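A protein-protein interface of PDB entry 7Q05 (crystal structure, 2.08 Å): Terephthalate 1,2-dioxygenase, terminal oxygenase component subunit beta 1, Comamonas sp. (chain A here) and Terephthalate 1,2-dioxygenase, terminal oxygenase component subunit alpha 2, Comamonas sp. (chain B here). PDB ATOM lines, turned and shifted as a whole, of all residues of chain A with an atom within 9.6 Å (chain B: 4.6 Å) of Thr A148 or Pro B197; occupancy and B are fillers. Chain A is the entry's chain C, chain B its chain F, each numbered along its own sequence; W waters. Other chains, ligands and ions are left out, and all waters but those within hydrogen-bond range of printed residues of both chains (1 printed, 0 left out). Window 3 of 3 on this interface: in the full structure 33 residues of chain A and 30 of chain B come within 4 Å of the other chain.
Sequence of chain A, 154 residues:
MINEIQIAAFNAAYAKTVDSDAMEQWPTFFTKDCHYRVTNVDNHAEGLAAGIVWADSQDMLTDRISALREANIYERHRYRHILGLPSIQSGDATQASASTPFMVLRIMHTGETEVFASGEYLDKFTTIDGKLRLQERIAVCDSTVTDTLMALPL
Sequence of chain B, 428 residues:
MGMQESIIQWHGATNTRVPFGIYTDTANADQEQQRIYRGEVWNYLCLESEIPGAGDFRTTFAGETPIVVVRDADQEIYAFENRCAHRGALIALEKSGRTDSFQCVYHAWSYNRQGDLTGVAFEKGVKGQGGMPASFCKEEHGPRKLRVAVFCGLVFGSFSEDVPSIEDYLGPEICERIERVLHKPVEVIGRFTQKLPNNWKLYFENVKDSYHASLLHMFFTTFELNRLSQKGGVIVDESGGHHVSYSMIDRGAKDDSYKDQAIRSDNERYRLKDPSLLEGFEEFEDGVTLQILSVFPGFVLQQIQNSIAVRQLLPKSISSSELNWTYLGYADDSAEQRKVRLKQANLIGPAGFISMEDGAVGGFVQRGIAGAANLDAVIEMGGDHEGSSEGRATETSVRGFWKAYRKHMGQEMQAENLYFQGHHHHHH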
ATOM      1  N   ILE A  73      16.291 -20.719 -12.047  1.00  0.00           N
ATOM      2  CA  ILE A  73      15.965 -19.380 -11.473  1.00  0.00           C
ATOM      3  C   ILE A  73      15.970 -19.532  -9.956  1.00  0.00           C
ATOM      4  O   ILE A  73      15.279 -20.439  -9.408  1.00  0.00           O
ATOM      5  CB  ILE A  73      14.641 -18.799 -12.017  1.00  0.00           C
ATOM      6  CG1 ILE A  73      14.818 -18.222 -13.435  1.00  0.00           C
ATOM      7  CG2 ILE A  73      14.031 -17.791 -11.046  1.00  0.00           C
ATOM      8  CD1 ILE A  73      16.215 -17.654 -13.739  1.00  0.00           C
ATOM      9  N   TYR A  74      16.823 -18.741  -9.309  1.00  0.00           N
ATOM     10  CA  TYR A  74      16.891 -18.658  -7.834  1.00  0.00           C
ATOM     11  C   TYR A  74      17.478 -17.290  -7.489  1.00  0.00           C
ATOM     12  O   TYR A  74      18.185 -16.680  -8.304  1.00  0.00           O
ATOM     13  CB  TYR A  74      17.643 -19.866  -7.289  1.00  0.00           C
ATOM     14  CG  TYR A  74      19.068 -19.956  -7.768  1.00  0.00           C
ATOM     15  CD1 TYR A  74      19.403 -20.555  -8.968  1.00  0.00           C
ATOM     16  CD2 TYR A  74      20.087 -19.421  -7.003  1.00  0.00           C
ATOM     17  CE1 TYR A  74      20.725 -20.625  -9.383  1.00  0.00           C
ATOM     18  CE2 TYR A  74      21.413 -19.507  -7.387  1.00  0.00           C
ATOM     19  CZ  TYR A  74      21.737 -20.127  -8.576  1.00  0.00           C
ATOM     20  OH  TYR A  74      23.049 -20.199  -8.959  1.00  0.00           O
ATOM     21  N   GLU A  75      17.087 -16.780  -6.331  1.00  0.00           N
ATOM     22  CA  GLU A  75      17.656 -15.542  -5.759  1.00  0.00           C
ATOM     23  C   GLU A  75      19.135 -15.808  -5.427  1.00  0.00           C
ATOM     24  O   GLU A  75      19.441 -16.901  -4.839  1.00  0.00           O
ATOM     25  CB  GLU A  75      16.845 -15.119  -4.533  1.00  0.00           C
ATOM     26  CG  GLU A  75      17.028 -13.648  -4.250  1.00  0.00           C
ATOM     27  CD  GLU A  75      16.147 -13.166  -3.119  1.00  0.00           C
ATOM     28  OE1 GLU A  75      15.446 -14.001  -2.541  1.00  0.00           O
ATOM     29  OE2 GLU A  75      16.285 -12.002  -2.756  1.00  0.00           O
ATOM     30  N   HIS A  77      22.570 -16.099  -3.742  1.00  0.00           N
ATOM     31  CA  HIS A  77      23.019 -16.420  -2.376  1.00  0.00           C
ATOM     32  C   HIS A  77      24.354 -17.138  -2.461  1.00  0.00           C
ATOM     33  O   HIS A  77      24.760 -17.489  -3.572  1.00  0.00           O
ATOM     34  CB  HIS A  77      21.963 -17.238  -1.647  1.00  0.00           C
ATOM     35  CG  HIS A  77      21.715 -18.590  -2.231  1.00  0.00           C
ATOM     36  ND1 HIS A  77      20.864 -18.795  -3.293  1.00  0.00           N
ATOM     37  CD2 HIS A  77      22.168 -19.814  -1.882  1.00  0.00           C
ATOM     38  CE1 HIS A  77      20.776 -20.094  -3.538  1.00  0.00           C
ATOM     39  NE2 HIS A  77      21.553 -20.735  -2.701  1.00  0.00           N
ATOM     40  N   TYR A  79      27.077 -19.954  -0.005  1.00  0.00           N
ATOM     41  CA  TYR A  79      27.306 -20.894   1.102  1.00  0.00           C
ATOM     42  C   TYR A  79      28.599 -20.528   1.819  1.00  0.00           C
ATOM     43  O   TYR A  79      29.523 -19.963   1.203  1.00  0.00           O
ATOM     44  CB  TYR A  79      27.405 -22.326   0.590  1.00  0.00           C
ATOM     45  CG  TYR A  79      26.121 -22.987   0.177  1.00  0.00           C
ATOM     46  CD1 TYR A  79      24.877 -22.447   0.449  1.00  0.00           C
ATOM     47  CD2 TYR A  79      26.175 -24.203  -0.491  1.00  0.00           C
ATOM     48  CE1 TYR A  79      23.716 -23.106   0.045  1.00  0.00           C
ATOM     49  CE2 TYR A  79      25.027 -24.857  -0.901  1.00  0.00           C
ATOM     50  CZ  TYR A  79      23.789 -24.305  -0.653  1.00  0.00           C
ATOM     51  OH  TYR A  79      22.677 -24.964  -1.101  1.00  0.00           O
ATOM     52  N   ARG A 106      23.815 -20.335   4.747  1.00  0.00           N
ATOM     53  CA  ARG A 106      23.406 -19.603   3.535  1.00  0.00           C
ATOM     54  C   ARG A 106      23.341 -18.118   3.861  1.00  0.00           C
ATOM     55  O   ARG A 106      22.748 -17.751   4.857  1.00  0.00           O
ATOM     56  CB  ARG A 106      22.089 -20.137   2.994  1.00  0.00           C
ATOM     57  CG  ARG A 106      21.592 -19.394   1.763  1.00  0.00           C
ATOM     58  CD  ARG A 106      20.224 -19.887   1.335  1.00  0.00           C
ATOM     59  NE  ARG A 106      19.258 -19.454   2.324  1.00  0.00           N
ATOM     60  CZ  ARG A 106      18.030 -19.876   2.392  1.00  0.00           C
ATOM     61  NH1 ARG A 106      17.576 -20.778   1.544  1.00  0.00           N
ATOM     62  NH2 ARG A 106      17.282 -19.411   3.350  1.00  0.00           N
ATOM     63  N   MET A 108      22.022 -14.822   1.863  1.00  0.00           N
ATOM     64  CA  MET A 108      21.323 -14.189   0.734  1.00  0.00           C
ATOM     65  C   MET A 108      22.108 -12.938   0.315  1.00  0.00           C
ATOM     66  O   MET A 108      22.768 -12.321   1.178  1.00  0.00           O
ATOM     67  CB  MET A 108      19.891 -13.800   1.162  1.00  0.00           C
ATOM     68  CG  MET A 108      19.023 -14.952   1.662  1.00  0.00           C
ATOM     69  SD  MET A 108      19.039 -16.375   0.519  1.00  0.00           S
ATOM     70  CE  MET A 108      18.294 -15.671  -0.938  1.00  0.00           C
ATOM     71  N   GLU A 114      21.622 -17.668   7.627  1.00  0.00           N
ATOM     72  CA  GLU A 114      20.960 -18.759   8.376  1.00  0.00           C
ATOM     73  C   GLU A 114      21.824 -20.008   8.359  1.00  0.00           C
ATOM     74  O   GLU A 114      22.531 -20.232   7.398  1.00  0.00           O
ATOM     75  CB  GLU A 114      19.614 -19.094   7.731  1.00  0.00           C
ATOM     76  CG  GLU A 114      18.560 -18.035   7.999  1.00  0.00           C
ATOM     77  CD  GLU A 114      17.419 -18.189   7.014  1.00  0.00           C
ATOM     78  OE1 GLU A 114      16.895 -19.358   6.901  1.00  0.00           O
ATOM     79  OE2 GLU A 114      17.128 -17.189   6.294  1.00  0.00           O
ATOM     80  N   PHE A 116      21.688 -23.291   7.117  1.00  0.00           N
ATOM     81  CA  PHE A 116      20.884 -23.842   6.013  1.00  0.00           C
ATOM     82  C   PHE A 116      20.919 -25.371   6.030  1.00  0.00           C
ATOM     83  O   PHE A 116      19.915 -25.974   5.630  1.00  0.00           O
ATOM     84  CB  PHE A 116      21.440 -23.291   4.705  1.00  0.00           C
ATOM     85  CG  PHE A 116      20.807 -23.881   3.475  1.00  0.00           C
ATOM     86  CD1 PHE A 116      19.541 -23.504   3.086  1.00  0.00           C
ATOM     87  CD2 PHE A 116      21.525 -24.739   2.658  1.00  0.00           C
ATOM     88  CE1 PHE A 116      18.968 -24.038   1.931  1.00  0.00           C
ATOM     89  CE2 PHE A 116      20.949 -25.297   1.535  1.00  0.00           C
ATOM     90  CZ  PHE A 116      19.671 -24.951   1.177  1.00  0.00           C
ATOM     91  N   VAL A 145      14.302 -30.585   6.648  1.00  0.00           N
ATOM     92  CA  VAL A 145      13.824 -29.295   6.104  1.00  0.00           C
ATOM     93  C   VAL A 145      14.946 -28.597   5.339  1.00  0.00           C
ATOM     94  O   VAL A 145      15.977 -28.411   5.893  1.00  0.00           O
ATOM     95  CB  VAL A 145      13.209 -28.411   7.203  1.00  0.00           C
ATOM     96  CG1 VAL A 145      12.712 -27.082   6.631  1.00  0.00           C
ATOM     97  CG2 VAL A 145      12.077 -29.152   7.909  1.00  0.00           C
ATOM     98  N   THR A 146      14.642 -28.201   4.086  1.00  0.00           N
ATOM     99  CA  THR A 146      15.397 -27.265   3.248  1.00  0.00           C
ATOM    100  C   THR A 146      14.602 -25.967   3.199  1.00  0.00           C
ATOM    101  O   THR A 146      13.425 -25.977   2.810  1.00  0.00           O
ATOM    102  CB  THR A 146      15.578 -27.800   1.828  1.00  0.00           C
ATOM    103  OG1 THR A 146      16.221 -29.064   1.877  1.00  0.00           O
ATOM    104  CG2 THR A 146      16.374 -26.846   0.964  1.00  0.00           C
ATOM    105  N   ASP A 147      15.220 -24.882   3.595  1.00  0.00           N
ATOM    106  CA  ASP A 147      14.566 -23.555   3.519  1.00  0.00           C
ATOM    107  C   ASP A 147      14.504 -23.109   2.051  1.00  0.00           C
ATOM    108  O   ASP A 147      15.573 -23.037   1.424  1.00  0.00           O
ATOM    109  CB  ASP A 147      15.268 -22.513   4.394  1.00  0.00           C
ATOM    110  CG  ASP A 147      14.464 -21.238   4.375  1.00  0.00           C
ATOM    111  OD1 ASP A 147      14.580 -20.520   3.392  1.00  0.00           O
ATOM    112  OD2 ASP A 147      13.581 -21.080   5.237  1.00  0.00           O
ATOM    113  N   THR A 148      13.285 -22.845   1.561  1.00  0.00           N
ATOM    114  CA  THR A 148      12.956 -22.339   0.206  1.00  0.00           C
ATOM    115  C   THR A 148      13.298 -23.353  -0.922  1.00  0.00           C
ATOM    116  O   THR A 148      12.405 -23.780  -1.599  1.00  0.00           O
ATOM    117  CB  THR A 148      13.673 -21.002  -0.030  1.00  0.00           C
ATOM    118  OG1 THR A 148      13.352 -20.127   1.037  1.00  0.00           O
ATOM    119  CG2 THR A 148      13.291 -20.377  -1.352  1.00  0.00           C
ATOM    120  N   LEU A 149      14.560 -23.586  -1.215  1.00  0.00           N
ATOM    121  CA  LEU A 149      15.053 -24.478  -2.308  1.00  0.00           C
ATOM    122  C   LEU A 149      16.529 -24.782  -2.031  1.00  0.00           C
ATOM    123  O   LEU A 149      17.097 -24.174  -1.119  1.00  0.00           O
ATOM    124  CB  LEU A 149      14.869 -23.826  -3.680  1.00  0.00           C
ATOM    125  CG  LEU A 149      15.529 -22.446  -3.850  1.00  0.00           C
ATOM    126  CD1 LEU A 149      17.026 -22.570  -4.091  1.00  0.00           C
ATOM    127  CD2 LEU A 149      14.914 -21.668  -4.985  1.00  0.00           C
ATOM    128  N   MET A 150      17.112 -25.699  -2.800  1.00  0.00           N
ATOM    129  CA  MET A 150      18.557 -26.029  -2.768  1.00  0.00           C
ATOM    130  C   MET A 150      19.096 -25.923  -4.191  1.00  0.00           C
ATOM    131  O   MET A 150      18.735 -26.767  -5.060  1.00  0.00           O
ATOM    132  CB  MET A 150      18.800 -27.421  -2.202  1.00  0.00           C
ATOM    133  CG  MET A 150      20.315 -27.715  -2.041  1.00  0.00           C
ATOM    134  SD  MET A 150      20.763 -29.246  -1.279  1.00  0.00           S
ATOM    135  CE  MET A 150      20.142 -28.990   0.376  1.00  0.00           C
ATOM    136  N   ALA A 151      19.896 -24.895  -4.463  1.00  0.00           N
ATOM    137  CA  ALA A 151      20.434 -24.622  -5.822  1.00  0.00           C
ATOM    138  C   ALA A 151      21.860 -25.174  -5.895  1.00  0.00           C
ATOM    139  O   ALA A 151      22.213 -25.797  -6.837  1.00  0.00           O
ATOM    140  CB  ALA A 151      20.424 -23.146  -6.128  1.00  0.00           C
ATOM    141  N   GLN B 194      10.210 -28.848   2.255  1.00  0.00           N
ATOM    142  CA  GLN B 194      10.627 -27.474   1.887  1.00  0.00           C
ATOM    143  C   GLN B 194       9.837 -26.508   2.766  1.00  0.00           C
ATOM    144  O   GLN B 194       8.632 -26.624   2.802  1.00  0.00           O
ATOM    145  CB  GLN B 194      10.235 -27.175   0.449  1.00  0.00           C
ATOM    146  CG  GLN B 194      11.328 -27.459  -0.510  1.00  0.00           C
ATOM    147  CD  GLN B 194      10.893 -27.254  -1.932  1.00  0.00           C
ATOM    148  OE1 GLN B 194      10.340 -28.161  -2.509  1.00  0.00           O
ATOM    149  NE2 GLN B 194      11.298 -26.155  -2.552  1.00  0.00           N
ATOM    150  N   LYS B 195      10.485 -25.616   3.481  1.00  0.00           N
ATOM    151  CA  LYS B 195       9.809 -24.475   4.141  1.00  0.00           C
ATOM    152  C   LYS B 195       9.741 -23.294   3.173  1.00  0.00           C
ATOM    153  O   LYS B 195      10.793 -22.817   2.687  1.00  0.00           O
ATOM    154  CB  LYS B 195      10.559 -24.111   5.406  1.00  0.00           C
ATOM    155  CG  LYS B 195       9.960 -23.009   6.269  1.00  0.00           C
ATOM    156  CD  LYS B 195      10.606 -23.146   7.643  1.00  0.00           C
ATOM    157  CE  LYS B 195      10.487 -21.921   8.499  1.00  0.00           C
ATOM    158  NZ  LYS B 195      11.777 -21.658   9.178  1.00  0.00           N
ATOM    159  N   LEU B 196       8.530 -22.904   2.805  1.00  0.00           N
ATOM    160  CA  LEU B 196       8.319 -21.909   1.730  1.00  0.00           C
ATOM    161  C   LEU B 196       8.094 -20.569   2.389  1.00  0.00           C
ATOM    162  O   LEU B 196       7.247 -20.455   3.274  1.00  0.00           O
ATOM    163  CB  LEU B 196       7.104 -22.303   0.920  1.00  0.00           C
ATOM    164  CG  LEU B 196       7.102 -23.690   0.306  1.00  0.00           C
ATOM    165  CD1 LEU B 196       5.770 -23.920  -0.361  1.00  0.00           C
ATOM    166  CD2 LEU B 196       8.231 -23.801  -0.647  1.00  0.00           C
ATOM    167  N   PRO B 197       8.825 -19.518   1.962  1.00  0.00           N
ATOM    168  CA  PRO B 197       8.630 -18.179   2.508  1.00  0.00           C
ATOM    169  C   PRO B 197       7.451 -17.473   1.832  1.00  0.00           C
ATOM    170  O   PRO B 197       7.566 -16.363   1.324  1.00  0.00           O
ATOM    171  CB  PRO B 197       9.977 -17.530   2.173  1.00  0.00           C
ATOM    172  CG  PRO B 197      10.274 -18.101   0.822  1.00  0.00           C
ATOM    173  CD  PRO B 197       9.881 -19.549   0.924  1.00  0.00           C
ATOM    174  N   ASN B 198       6.300 -18.119   1.854  1.00  0.00           N
ATOM    175  CA  ASN B 198       5.069 -17.554   1.252  1.00  0.00           C
ATOM    176  C   ASN B 198       3.857 -18.152   1.945  1.00  0.00           C
ATOM    177  O   ASN B 198       3.929 -19.292   2.502  1.00  0.00           O
ATOM    178  CB  ASN B 198       5.067 -17.737  -0.253  1.00  0.00           C
ATOM    179  CG  ASN B 198       5.263 -19.169  -0.697  1.00  0.00           C
ATOM    180  OD1 ASN B 198       6.346 -19.547  -1.148  1.00  0.00           O
ATOM    181  ND2 ASN B 198       4.231 -19.976  -0.574  1.00  0.00           N
ATOM    182  N   SER B 319       2.845 -15.774   6.230  1.00  0.00           N
ATOM    183  CA  SER B 319       3.822 -15.655   5.117  1.00  0.00           C
ATOM    184  C   SER B 319       4.778 -16.853   5.080  1.00  0.00           C
ATOM    185  O   SER B 319       5.876 -16.696   4.527  1.00  0.00           O
ATOM    186  CB  SER B 319       4.561 -14.359   5.187  1.00  0.00           C
ATOM    187  OG  SER B 319       5.140 -14.252   6.464  1.00  0.00           O
ATOM    188  N   GLY B 359       9.802 -23.381  -5.375  1.00  0.00           N
ATOM    189  CA  GLY B 359      10.055 -23.044  -3.965  1.00  0.00           C
ATOM    190  C   GLY B 359      10.239 -21.539  -3.749  1.00  0.00           C
ATOM    191  O   GLY B 359      10.046 -21.117  -2.609  1.00  0.00           O
ATOM    192  N   ALA B 360      10.614 -20.764  -4.760  1.00  0.00           N
ATOM    193  CA  ALA B 360      10.980 -19.353  -4.587  1.00  0.00           C
ATOM    194  C   ALA B 360       9.909 -18.378  -5.131  1.00  0.00           C
ATOM    195  O   ALA B 360       9.932 -17.192  -4.645  1.00  0.00           O
ATOM    196  CB  ALA B 360      12.322 -19.077  -5.255  1.00  0.00           C
ATOM    197  N   GLY B 363       7.511 -16.515  -2.856  1.00  0.00           N
ATOM    198  CA  GLY B 363       8.151 -15.478  -2.039  1.00  0.00           C
ATOM    199  C   GLY B 363       8.376 -14.249  -2.863  1.00  0.00           C
ATOM    200  O   GLY B 363       8.306 -13.158  -2.295  1.00  0.00           O
ATOM    201  N   GLN B 366       5.029 -12.664  -2.569  1.00  0.00           N
ATOM    202  CA  GLN B 366       4.882 -12.209  -1.177  1.00  0.00           C
ATOM    203  C   GLN B 366       5.611 -10.865  -1.020  1.00  0.00           C
ATOM    204  O   GLN B 366       5.012  -9.917  -0.435  1.00  0.00           O
ATOM    205  CB  GLN B 366       5.344 -13.296  -0.196  1.00  0.00           C
ATOM    206  CG  GLN B 366       4.865 -13.040   1.223  1.00  0.00           C
ATOM    207  CD  GLN B 366       3.509 -13.628   1.505  1.00  0.00           C
ATOM    208  OE1 GLN B 366       3.179 -14.732   1.113  1.00  0.00           O
ATOM    209  NE2 GLN B 366       2.699 -12.897   2.247  1.00  0.00           N
HETATM  210  O   HOH W   1      11.174 -20.304   4.086  1.00  0.00           O
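Of the printed residues of chain B, Val A145 touches Lys B195 (3.9 Å).
Thr A148 touches just these residues of chain B: Gln B194, Lys B195, Pro B197 and Gly B359.
Of the printed residues of chain B, Leu A149 touches Ala B360 (3.7 Å).
Of the printed residues of chain A, Lys B195 touches Val A145 (3.9 Å), Thr A146 (3.0 Å), Asp A147 (3.8 Å) and Thr A148 (2.7 Å).
Leu B196 touches none of the printed residues of chain A.
Pro B197 touches just one residue of chain A: Thr A148.
No residue of chain A comes within 4 Å of Asn B198.
Of the printed residues of chain A, Gly B359 touches Thr A148.
No residue of chain A comes within 4 Å of Gly B363.
Gln B366 touches none of the printed residues of chain A.
The nearest residue of chain B that does not touch Thr A148 is Ala B360 (4.1 Å).
N of Lys B195 lies within hydrogen-bond range of O of Thr A146, 3.0 Å away.
The backbone carbonyl oxygen (O) of Thr A148 sits at hydrogen-bond distance from the side-chain amide nitrogen (NE2) of Gln B194, 2.8 Å away.
The backbone NH (N) of Thr A148 sits at hydrogen-bond distance from the backbone carbonyl oxygen (O) of Lys B195 (2.7 Å).
Water W1 bridges the side-chain carboxylate (OD2) of Asp A147 (2.8 Å) and the backbone carbonyl oxygen (O) of Lys B195 (2.9 Å).
Of the 16 printed residues of chain A, 5 touch a printed residue of chain B.
Hydrophobic or aromatic side chains of chain A within 4 Å of the printed part of chain B: Val A145 and Leu A149.
Among the printed residues, 9 pairs touch across the chains.
Among the printed residues, no Asp or Glu carboxylate lies within 4 Å of a Lys or Arg side-chain nitrogen of the other chain.
Among the printed residues, pairs that only touch across the chains: Thr A146 with Gln B194, Thr A148 with Gly B359, Thr A148 with Pro B197, Leu A149 with Ala B360, Asp A147 with Lys B195 and Val A145 with Lys B195.
The guanidinium group (NH2) of Arg A106 lies within salt-bridge range of the side-chain carboxylate (OD1) of Asp A147.
OD1 of Asp A147 lies within hydrogen-bond range of OG1 of Thr A148 (2.7 Å).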
